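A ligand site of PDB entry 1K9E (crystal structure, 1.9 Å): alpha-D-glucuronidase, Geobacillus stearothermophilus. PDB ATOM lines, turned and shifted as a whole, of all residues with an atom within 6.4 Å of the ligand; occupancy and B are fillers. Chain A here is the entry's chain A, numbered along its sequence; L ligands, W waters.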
ATOM      1  N   TRP A 150       6.401 -12.840  -3.598  1.00  0.00           N
ATOM      2  CA  TRP A 150       5.084 -13.247  -4.042  1.00  0.00           C
ATOM      3  C   TRP A 150       4.288 -12.017  -4.481  1.00  0.00           C
ATOM      4  O   TRP A 150       3.055 -12.006  -4.488  1.00  0.00           O
ATOM      5  CB  TRP A 150       4.367 -14.018  -2.940  1.00  0.00           C
ATOM      6  CG  TRP A 150       4.896 -15.431  -2.798  1.00  0.00           C
ATOM      7  CD1 TRP A 150       5.925 -15.995  -3.501  1.00  0.00           C
ATOM      8  CD2 TRP A 150       4.431 -16.437  -1.898  1.00  0.00           C
ATOM      9  NE1 TRP A 150       6.128 -17.294  -3.094  1.00  0.00           N
ATOM     10  CE2 TRP A 150       5.221 -17.598  -2.110  1.00  0.00           C
ATOM     11  CE3 TRP A 150       3.420 -16.485  -0.928  1.00  0.00           C
ATOM     12  CZ2 TRP A 150       5.040 -18.776  -1.392  1.00  0.00           C
ATOM     13  CZ3 TRP A 150       3.230 -17.663  -0.213  1.00  0.00           C
ATOM     14  CH2 TRP A 150       4.036 -18.794  -0.452  1.00  0.00           C
ATOM     15  N   GLU A 158       0.788 -11.644  -2.589  1.00  0.00           N
ATOM     16  CA  GLU A 158       0.079 -12.814  -2.062  1.00  0.00           C
ATOM     17  C   GLU A 158       0.712 -13.172  -0.726  1.00  0.00           C
ATOM     18  O   GLU A 158       1.915 -13.372  -0.620  1.00  0.00           O
ATOM     19  CB  GLU A 158       0.169 -13.992  -3.039  1.00  0.00           C
ATOM     20  CG  GLU A 158      -0.824 -15.090  -2.694  1.00  0.00           C
ATOM     21  CD  GLU A 158      -1.025 -16.096  -3.814  1.00  0.00           C
ATOM     22  OE1 GLU A 158      -0.878 -15.716  -4.999  1.00  0.00           O
ATOM     23  OE2 GLU A 158      -1.354 -17.264  -3.508  1.00  0.00           O
ATOM     24  N   ARG A 159      -0.129 -13.240   0.306  1.00  0.00           N
ATOM     25  CA  ARG A 159       0.336 -13.536   1.664  1.00  0.00           C
ATOM     26  C   ARG A 159       1.316 -12.453   2.130  1.00  0.00           C
ATOM     27  O   ARG A 159       2.315 -12.745   2.792  1.00  0.00           O
ATOM     28  CB  ARG A 159       0.992 -14.915   1.728  1.00  0.00           C
ATOM     29  CG  ARG A 159       0.171 -16.036   1.091  1.00  0.00           C
ATOM     30  CD  ARG A 159      -1.247 -16.126   1.646  1.00  0.00           C
ATOM     31  NE  ARG A 159      -2.016 -17.166   0.961  1.00  0.00           N
ATOM     32  CZ  ARG A 159      -3.288 -17.450   1.208  1.00  0.00           C
ATOM     33  NH1 ARG A 159      -3.961 -16.772   2.132  1.00  0.00           N
ATOM     34  NH2 ARG A 159      -3.886 -18.421   0.532  1.00  0.00           N
ATOM     35  N   ASN A 199       5.549 -13.050  -8.053  1.00  0.00           N
ATOM     36  CA  ASN A 199       4.778 -14.162  -7.505  1.00  0.00           C
ATOM     37  C   ASN A 199       4.940 -15.470  -8.280  1.00  0.00           C
ATOM     38  O   ASN A 199       4.936 -15.479  -9.514  1.00  0.00           O
ATOM     39  CB  ASN A 199       3.296 -13.761  -7.489  1.00  0.00           C
ATOM     40  CG  ASN A 199       2.443 -14.677  -6.635  1.00  0.00           C
ATOM     41  OD1 ASN A 199       2.910 -15.701  -6.152  1.00  0.00           O
ATOM     42  ND2 ASN A 199       1.192 -14.290  -6.445  1.00  0.00           N
ATOM     43  N   VAL A 200       5.067 -16.583  -7.554  1.00  0.00           N
ATOM     44  CA  VAL A 200       5.208 -17.888  -8.190  1.00  0.00           C
ATOM     45  C   VAL A 200       3.898 -18.234  -8.914  1.00  0.00           C
ATOM     46  O   VAL A 200       3.875 -19.055  -9.827  1.00  0.00           O
ATOM     47  CB  VAL A 200       5.565 -18.971  -7.154  1.00  0.00           C
ATOM     48  CG1 VAL A 200       6.975 -18.706  -6.607  1.00  0.00           C
ATOM     49  CG2 VAL A 200       4.564 -18.993  -6.015  1.00  0.00           C
ATOM     50  N   ASN A 201       2.801 -17.602  -8.483  1.00  0.00           N
ATOM     51  CA  ASN A 201       1.507 -17.775  -9.154  1.00  0.00           C
ATOM     52  C   ASN A 201       1.538 -16.633 -10.167  1.00  0.00           C
ATOM     53  O   ASN A 201       1.177 -15.499  -9.846  1.00  0.00           O
ATOM     54  CB  ASN A 201       0.322 -17.572  -8.210  1.00  0.00           C
ATOM     55  CG  ASN A 201       0.103 -18.735  -7.264  1.00  0.00           C
ATOM     56  OD1 ASN A 201       0.308 -19.888  -7.621  1.00  0.00           O
ATOM     57  ND2 ASN A 201      -0.354 -18.428  -6.049  1.00  0.00           N
ATOM     58  N   LYS A 281       6.401 -22.818 -10.692  1.00  0.00           N
ATOM     59  CA  LYS A 281       5.346 -23.486  -9.945  1.00  0.00           C
ATOM     60  C   LYS A 281       4.407 -23.996 -11.035  1.00  0.00           C
ATOM     61  O   LYS A 281       3.678 -23.218 -11.645  1.00  0.00           O
ATOM     62  CB  LYS A 281       4.596 -22.521  -9.028  1.00  0.00           C
ATOM     63  CG  LYS A 281       3.416 -23.187  -8.318  1.00  0.00           C
ATOM     64  CD  LYS A 281       2.700 -22.240  -7.370  1.00  0.00           C
ATOM     65  CE  LYS A 281       1.480 -22.909  -6.735  1.00  0.00           C
ATOM     66  NZ  LYS A 281       0.794 -22.010  -5.777  1.00  0.00           N
ATOM     67  N   ARG A 318       9.810 -25.890  -8.126  1.00  0.00           N
ATOM     68  CA  ARG A 318       9.186 -26.089  -6.817  1.00  0.00           C
ATOM     69  C   ARG A 318       8.450 -27.414  -6.725  1.00  0.00           C
ATOM     70  O   ARG A 318       7.722 -27.797  -7.639  1.00  0.00           O
ATOM     71  CB  ARG A 318       8.235 -24.933  -6.518  1.00  0.00           C
ATOM     72  CG  ARG A 318       8.927 -23.586  -6.468  1.00  0.00           C
ATOM     73  CD  ARG A 318       7.957 -22.471  -6.132  1.00  0.00           C
ATOM     74  NE  ARG A 318       7.600 -22.423  -4.715  1.00  0.00           N
ATOM     75  CZ  ARG A 318       6.347 -22.499  -4.257  1.00  0.00           C
ATOM     76  NH1 ARG A 318       5.334 -22.634  -5.104  1.00  0.00           N
ATOM     77  NH2 ARG A 318       6.116 -22.369  -2.960  1.00  0.00           N
ATOM     78  N   PHE A 320       6.216 -28.140  -4.452  1.00  0.00           N
ATOM     79  CA  PHE A 320       4.970 -27.976  -3.714  1.00  0.00           C
ATOM     80  C   PHE A 320       3.869 -28.449  -4.655  1.00  0.00           C
ATOM     81  O   PHE A 320       3.188 -27.640  -5.293  1.00  0.00           O
ATOM     82  CB  PHE A 320       4.760 -26.512  -3.332  1.00  0.00           C
ATOM     83  CG  PHE A 320       3.562 -26.282  -2.454  1.00  0.00           C
ATOM     84  CD1 PHE A 320       3.427 -26.972  -1.251  1.00  0.00           C
ATOM     85  CD2 PHE A 320       2.575 -25.379  -2.820  1.00  0.00           C
ATOM     86  CE1 PHE A 320       2.308 -26.759  -0.423  1.00  0.00           C
ATOM     87  CE2 PHE A 320       1.461 -25.156  -2.012  1.00  0.00           C
ATOM     88  CZ  PHE A 320       1.335 -25.846  -0.805  1.00  0.00           C
ATOM     89  N   TYR A 322       0.620 -31.442  -5.075  1.00  0.00           N
ATOM     90  CA  TYR A 322      -0.253 -32.363  -4.362  1.00  0.00           C
ATOM     91  C   TYR A 322      -1.645 -32.369  -4.982  1.00  0.00           C
ATOM     92  O   TYR A 322      -1.982 -31.509  -5.798  1.00  0.00           O
ATOM     93  CB  TYR A 322      -0.353 -31.941  -2.895  1.00  0.00           C
ATOM     94  CG  TYR A 322      -0.954 -30.562  -2.693  1.00  0.00           C
ATOM     95  CD1 TYR A 322      -2.330 -30.384  -2.600  1.00  0.00           C
ATOM     96  CD2 TYR A 322      -0.133 -29.438  -2.610  1.00  0.00           C
ATOM     97  CE1 TYR A 322      -2.892 -29.114  -2.436  1.00  0.00           C
ATOM     98  CE2 TYR A 322      -0.682 -28.167  -2.452  1.00  0.00           C
ATOM     99  CZ  TYR A 322      -2.058 -28.010  -2.359  1.00  0.00           C
ATOM    100  OH  TYR A 322      -2.587 -26.748  -2.195  1.00  0.00           O
ATOM    101  N   ARG A 335      -1.658 -36.392   1.863  1.00  0.00           N
ATOM    102  CA  ARG A 335      -0.999 -35.270   1.197  1.00  0.00           C
ATOM    103  C   ARG A 335       0.468 -35.168   1.587  1.00  0.00           C
ATOM    104  O   ARG A 335       1.306 -34.772   0.778  1.00  0.00           O
ATOM    105  CB  ARG A 335      -1.719 -33.962   1.532  1.00  0.00           C
ATOM    106  CG  ARG A 335      -1.029 -32.724   0.988  1.00  0.00           C
ATOM    107  CD  ARG A 335      -1.847 -31.463   1.242  1.00  0.00           C
ATOM    108  NE  ARG A 335      -1.070 -30.273   0.935  1.00  0.00           N
ATOM    109  CZ  ARG A 335      -1.544 -29.032   0.990  1.00  0.00           C
ATOM    110  NH1 ARG A 335      -2.802 -28.811   1.337  1.00  0.00           N
ATOM    111  NH2 ARG A 335      -0.752 -28.002   0.700  1.00  0.00           N
ATOM    112  N   LYS A 359       9.801 -27.189   0.304  1.00  0.00           N
ATOM    113  CA  LYS A 359       9.451 -26.506   1.545  1.00  0.00           C
ATOM    114  C   LYS A 359      10.029 -27.283   2.725  1.00  0.00           C
ATOM    115  O   LYS A 359      10.232 -28.498   2.630  1.00  0.00           O
ATOM    116  CB  LYS A 359       7.929 -26.384   1.678  1.00  0.00           C
ATOM    117  CG  LYS A 359       7.312 -25.372   0.722  1.00  0.00           C
ATOM    118  CD  LYS A 359       5.821 -25.155   0.978  1.00  0.00           C
ATOM    119  CE  LYS A 359       5.246 -24.111   0.014  1.00  0.00           C
ATOM    120  NZ  LYS A 359       3.814 -23.790   0.296  1.00  0.00           N
ATOM    121  N   ASP A 364       2.417 -27.554   4.399  1.00  0.00           N
ATOM    122  CA  ASP A 364       2.408 -26.177   3.924  1.00  0.00           C
ATOM    123  C   ASP A 364       2.714 -25.099   4.959  1.00  0.00           C
ATOM    124  O   ASP A 364       1.816 -24.415   5.449  1.00  0.00           O
ATOM    125  CB  ASP A 364       1.072 -25.872   3.232  1.00  0.00           C
ATOM    126  CG  ASP A 364       1.026 -24.471   2.631  1.00  0.00           C
ATOM    127  OD1 ASP A 364       2.095 -23.899   2.307  1.00  0.00           O
ATOM    128  OD2 ASP A 364      -0.093 -23.939   2.461  1.00  0.00           O
ATOM    129  N   PHE A 365       4.002 -24.947   5.273  1.00  0.00           N
ATOM    130  CA  PHE A 365       4.478 -23.924   6.204  1.00  0.00           C
ATOM    131  C   PHE A 365       3.699 -23.780   7.513  1.00  0.00           C
ATOM    132  O   PHE A 365       3.483 -22.664   7.982  1.00  0.00           O
ATOM    133  CB  PHE A 365       4.502 -22.552   5.520  1.00  0.00           C
ATOM    134  CG  PHE A 365       5.416 -22.476   4.311  1.00  0.00           C
ATOM    135  CD1 PHE A 365       6.715 -22.983   4.368  1.00  0.00           C
ATOM    136  CD2 PHE A 365       5.003 -21.810   3.161  1.00  0.00           C
ATOM    137  CE1 PHE A 365       7.594 -22.824   3.293  1.00  0.00           C
ATOM    138  CE2 PHE A 365       5.872 -21.642   2.084  1.00  0.00           C
ATOM    139  CZ  PHE A 365       7.168 -22.149   2.150  1.00  0.00           C
ATOM    140  N   GLU A 386      12.978 -24.307   0.809  1.00  0.00           N
ATOM    141  CA  GLU A 386      12.209 -23.073   0.765  1.00  0.00           C
ATOM    142  C   GLU A 386      11.576 -22.890   2.137  1.00  0.00           C
ATOM    143  O   GLU A 386      10.921 -23.797   2.644  1.00  0.00           O
ATOM    144  CB  GLU A 386      11.097 -23.169  -0.281  1.00  0.00           C
ATOM    145  CG  GLU A 386      10.297 -21.891  -0.471  1.00  0.00           C
ATOM    146  CD  GLU A 386       9.128 -22.067  -1.417  1.00  0.00           C
ATOM    147  OE1 GLU A 386       9.282 -22.812  -2.413  1.00  0.00           O
ATOM    148  OE2 GLU A 386       8.058 -21.469  -1.176  1.00  0.00           O
ATOM    149  N   GLN A 388       9.369 -19.941   4.701  1.00  0.00           N
ATOM    150  CA  GLN A 388       8.490 -18.796   4.520  1.00  0.00           C
ATOM    151  C   GLN A 388       8.759 -17.729   5.576  1.00  0.00           C
ATOM    152  O   GLN A 388       8.477 -17.936   6.759  1.00  0.00           O
ATOM    153  CB  GLN A 388       7.028 -19.266   4.567  1.00  0.00           C
ATOM    154  CG  GLN A 388       6.025 -18.216   4.121  1.00  0.00           C
ATOM    155  CD  GLN A 388       4.590 -18.734   4.155  1.00  0.00           C
ATOM    156  OE1 GLN A 388       4.151 -19.284   5.160  1.00  0.00           O
ATOM    157  NE2 GLN A 388       3.878 -18.552   3.049  1.00  0.00           N
ATOM    158  N   GLU A 392       2.488 -16.439   7.086  1.00  0.00           N
ATOM    159  CA  GLU A 392       1.159 -16.866   6.681  1.00  0.00           C
ATOM    160  C   GLU A 392       0.401 -17.650   7.750  1.00  0.00           C
ATOM    161  O   GLU A 392      -0.745 -17.344   8.056  1.00  0.00           O
ATOM    162  CB  GLU A 392       1.217 -17.694   5.396  1.00  0.00           C
ATOM    163  CG  GLU A 392      -0.142 -18.213   4.972  1.00  0.00           C
ATOM    164  CD  GLU A 392      -0.134 -18.896   3.618  1.00  0.00           C
ATOM    165  OE1 GLU A 392       0.953 -19.023   3.019  1.00  0.00           O
ATOM    166  OE2 GLU A 392      -1.227 -19.304   3.158  1.00  0.00           O
ATOM    167  N   TYR A 393       1.038 -18.674   8.294  1.00  0.00           N
ATOM    168  CA  TYR A 393       0.400 -19.494   9.316  1.00  0.00           C
ATOM    169  C   TYR A 393       1.034 -19.261  10.674  1.00  0.00           C
ATOM    170  O   TYR A 393       0.698 -19.948  11.640  1.00  0.00           O
ATOM    171  CB  TYR A 393       0.541 -20.971   8.955  1.00  0.00           C
ATOM    172  CG  TYR A 393      -0.099 -21.323   7.640  1.00  0.00           C
ATOM    173  CD1 TYR A 393      -1.488 -21.413   7.513  1.00  0.00           C
ATOM    174  CD2 TYR A 393       0.676 -21.602   6.510  1.00  0.00           C
ATOM    175  CE1 TYR A 393      -2.080 -21.770   6.317  1.00  0.00           C
ATOM    176  CE2 TYR A 393       0.087 -21.958   5.303  1.00  0.00           C
ATOM    177  CZ  TYR A 393      -1.292 -22.047   5.212  1.00  0.00           C
ATOM    178  OH  TYR A 393      -1.889 -22.413   4.034  1.00  0.00           O
ATOM    179  N   VAL A 443      10.642 -16.949   1.368  1.00  0.00           N
ATOM    180  CA  VAL A 443       9.543 -16.147   0.834  1.00  0.00           C
ATOM    181  C   VAL A 443       9.520 -14.832   1.599  1.00  0.00           C
ATOM    182  O   VAL A 443       9.258 -14.787   2.805  1.00  0.00           O
ATOM    183  CB  VAL A 443       8.192 -16.877   1.013  1.00  0.00           C
ATOM    184  CG1 VAL A 443       7.060 -16.058   0.416  1.00  0.00           C
ATOM    185  CG2 VAL A 443       8.263 -18.257   0.347  1.00  0.00           C
ATOM    186  N   GLY A 525      -9.134 -19.569   3.551  1.00  0.00           N
ATOM    187  CA  GLY A 525      -8.966 -18.364   2.766  1.00  0.00           C
ATOM    188  C   GLY A 525      -7.783 -17.532   3.194  1.00  0.00           C
ATOM    189  O   GLY A 525      -6.682 -17.707   2.663  1.00  0.00           O
ATOM    190  N   HIS A 527      -6.375 -17.571   6.201  1.00  0.00           N
ATOM    191  CA  HIS A 527      -5.552 -18.355   7.121  1.00  0.00           C
ATOM    192  C   HIS A 527      -5.152 -17.733   8.454  1.00  0.00           C
ATOM    193  O   HIS A 527      -4.239 -18.219   9.125  1.00  0.00           O
ATOM    194  CB  HIS A 527      -4.300 -18.828   6.390  1.00  0.00           C
ATOM    195  CG  HIS A 527      -4.593 -19.671   5.197  1.00  0.00           C
ATOM    196  ND1 HIS A 527      -3.678 -19.889   4.182  1.00  0.00           N
ATOM    197  CD2 HIS A 527      -5.701 -20.366   4.843  1.00  0.00           C
ATOM    198  CE1 HIS A 527      -4.216 -20.675   3.270  1.00  0.00           C
ATOM    199  NE2 HIS A 527      -5.442 -20.972   3.646  1.00  0.00           N
HETATM  200  C1  LIG L   1       1.707 -18.542  -3.877  1.00  0.00           C
HETATM  201  C2  LIG L   1       0.171 -21.867   0.082  1.00  0.00           C
HETATM  202  C3  LIG L   1      -0.204 -20.381   0.142  1.00  0.00           C
HETATM  203  C4  LIG L   1      -0.142 -19.905  -1.404  1.00  0.00           C
HETATM  204  C5  LIG L   1       1.076 -20.053  -2.224  1.00  0.00           C
HETATM  205  C6  LIG L   1       1.602 -21.325  -1.751  1.00  0.00           C
HETATM  206  C7  LIG L   1       2.807 -21.770  -2.435  1.00  0.00           C
HETATM  207  O1  LIG L   1      -0.828 -22.691  -0.405  1.00  0.00           O
HETATM  208  O2  LIG L   1      -1.464 -20.179   0.813  1.00  0.00           O
HETATM  209  O3  LIG L   1      -0.594 -18.557  -1.166  1.00  0.00           O
HETATM  210  O4  LIG L   1       0.778 -19.598  -3.545  1.00  0.00           O
HETATM  211  O5  LIG L   1       1.379 -22.222  -0.633  1.00  0.00           O
HETATM  212  O6  LIG L   1       2.651 -21.940  -3.796  1.00  0.00           O
HETATM  213  O7  LIG L   1       3.881 -21.953  -1.626  1.00  0.00           O
HETATM  214  O   HOH W   1      -3.581 -21.703  -0.481  1.00  0.00           O
HETATM  215  O   HOH W   2      -1.865 -21.423  -4.700  1.00  0.00           O
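The side-chain amino group of Lys 281 is in salt-bridge range of an oxygen (O6) of the ligand (2.7 Å).
An oxygen (O2) of the ligand is in hydrogen-bond range of the side-chain carboxylate (OE2) of Glu 392.
The side-chain amide nitrogen (ND2) of Asn 201 sits at hydrogen-bond distance from an oxygen (O4) of the ligand, at 3.0 Å.
The guanidinium group (NH2) of Arg 318 lies within salt-bridge range of an oxygen (O7) of the ligand.
The side-chain carboxylate (OD2) of Asp 364 lies close to an oxygen (O1) of the ligand (3.2 Å).
O7 of the ligand lies within salt-bridge range of NZ of Lys 359, 2.7 Å away.
The side-chain carboxylate (OE2) of Glu 158 lies within hydrogen-bond range of an oxygen (O3) of the ligand (2.8 Å).
An oxygen (O3) of the ligand is in hydrogen-bond range of the guanidinium group (NE) of Arg 159 (2.9 Å).
The side-chain amino group of Lys 359 is in salt-bridge range of the side-chain carboxylate of Asp 364.
N of Glu 158 sits at hydrogen-bond distance from O of Trp 150, 3.0 Å away.
The guanidinium group of Arg 318 is in salt-bridge range of the side-chain carboxylate of Glu 386, 2.8 Å away.
The side-chain amide nitrogen (ND2) of Asn 201 is in hydrogen-bond range of the side-chain carboxylate (OE1) of Glu 158, 3.0 Å away.
The backbone carbonyl oxygen of Gly 525 is in hydrogen-bond range of the guanidinium group of Arg 159.
OD2 of Asp 364 is in hydrogen-bond range of OH of Tyr 393 (2.8 Å).
The side-chain amino group of Lys 281 is in hydrogen-bond range of the side-chain amide oxygen of Asn 201 (2.9 Å).
NE of Arg 159 lies within salt-bridge range of OE2 of Glu 392, 3.2 Å away.
Residues that only touch the ligand: Phe 320, Trp 150, Val 200, His 527, Asn 199 and Tyr 393.
Of the 21 residues printed, 14 come within 4 Å of the ligand.
The nearest printed residue that does not touch the ligand is Phe 365 (4.2 Å).
Water W1 lies within hydrogen-bond range of O2 of the ligand (2.9 Å) and NH2 of Arg 159 (3.4 Å).
Water W2 lies within hydrogen-bond range of NZ of Lys 281 and O4 of the ligand.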
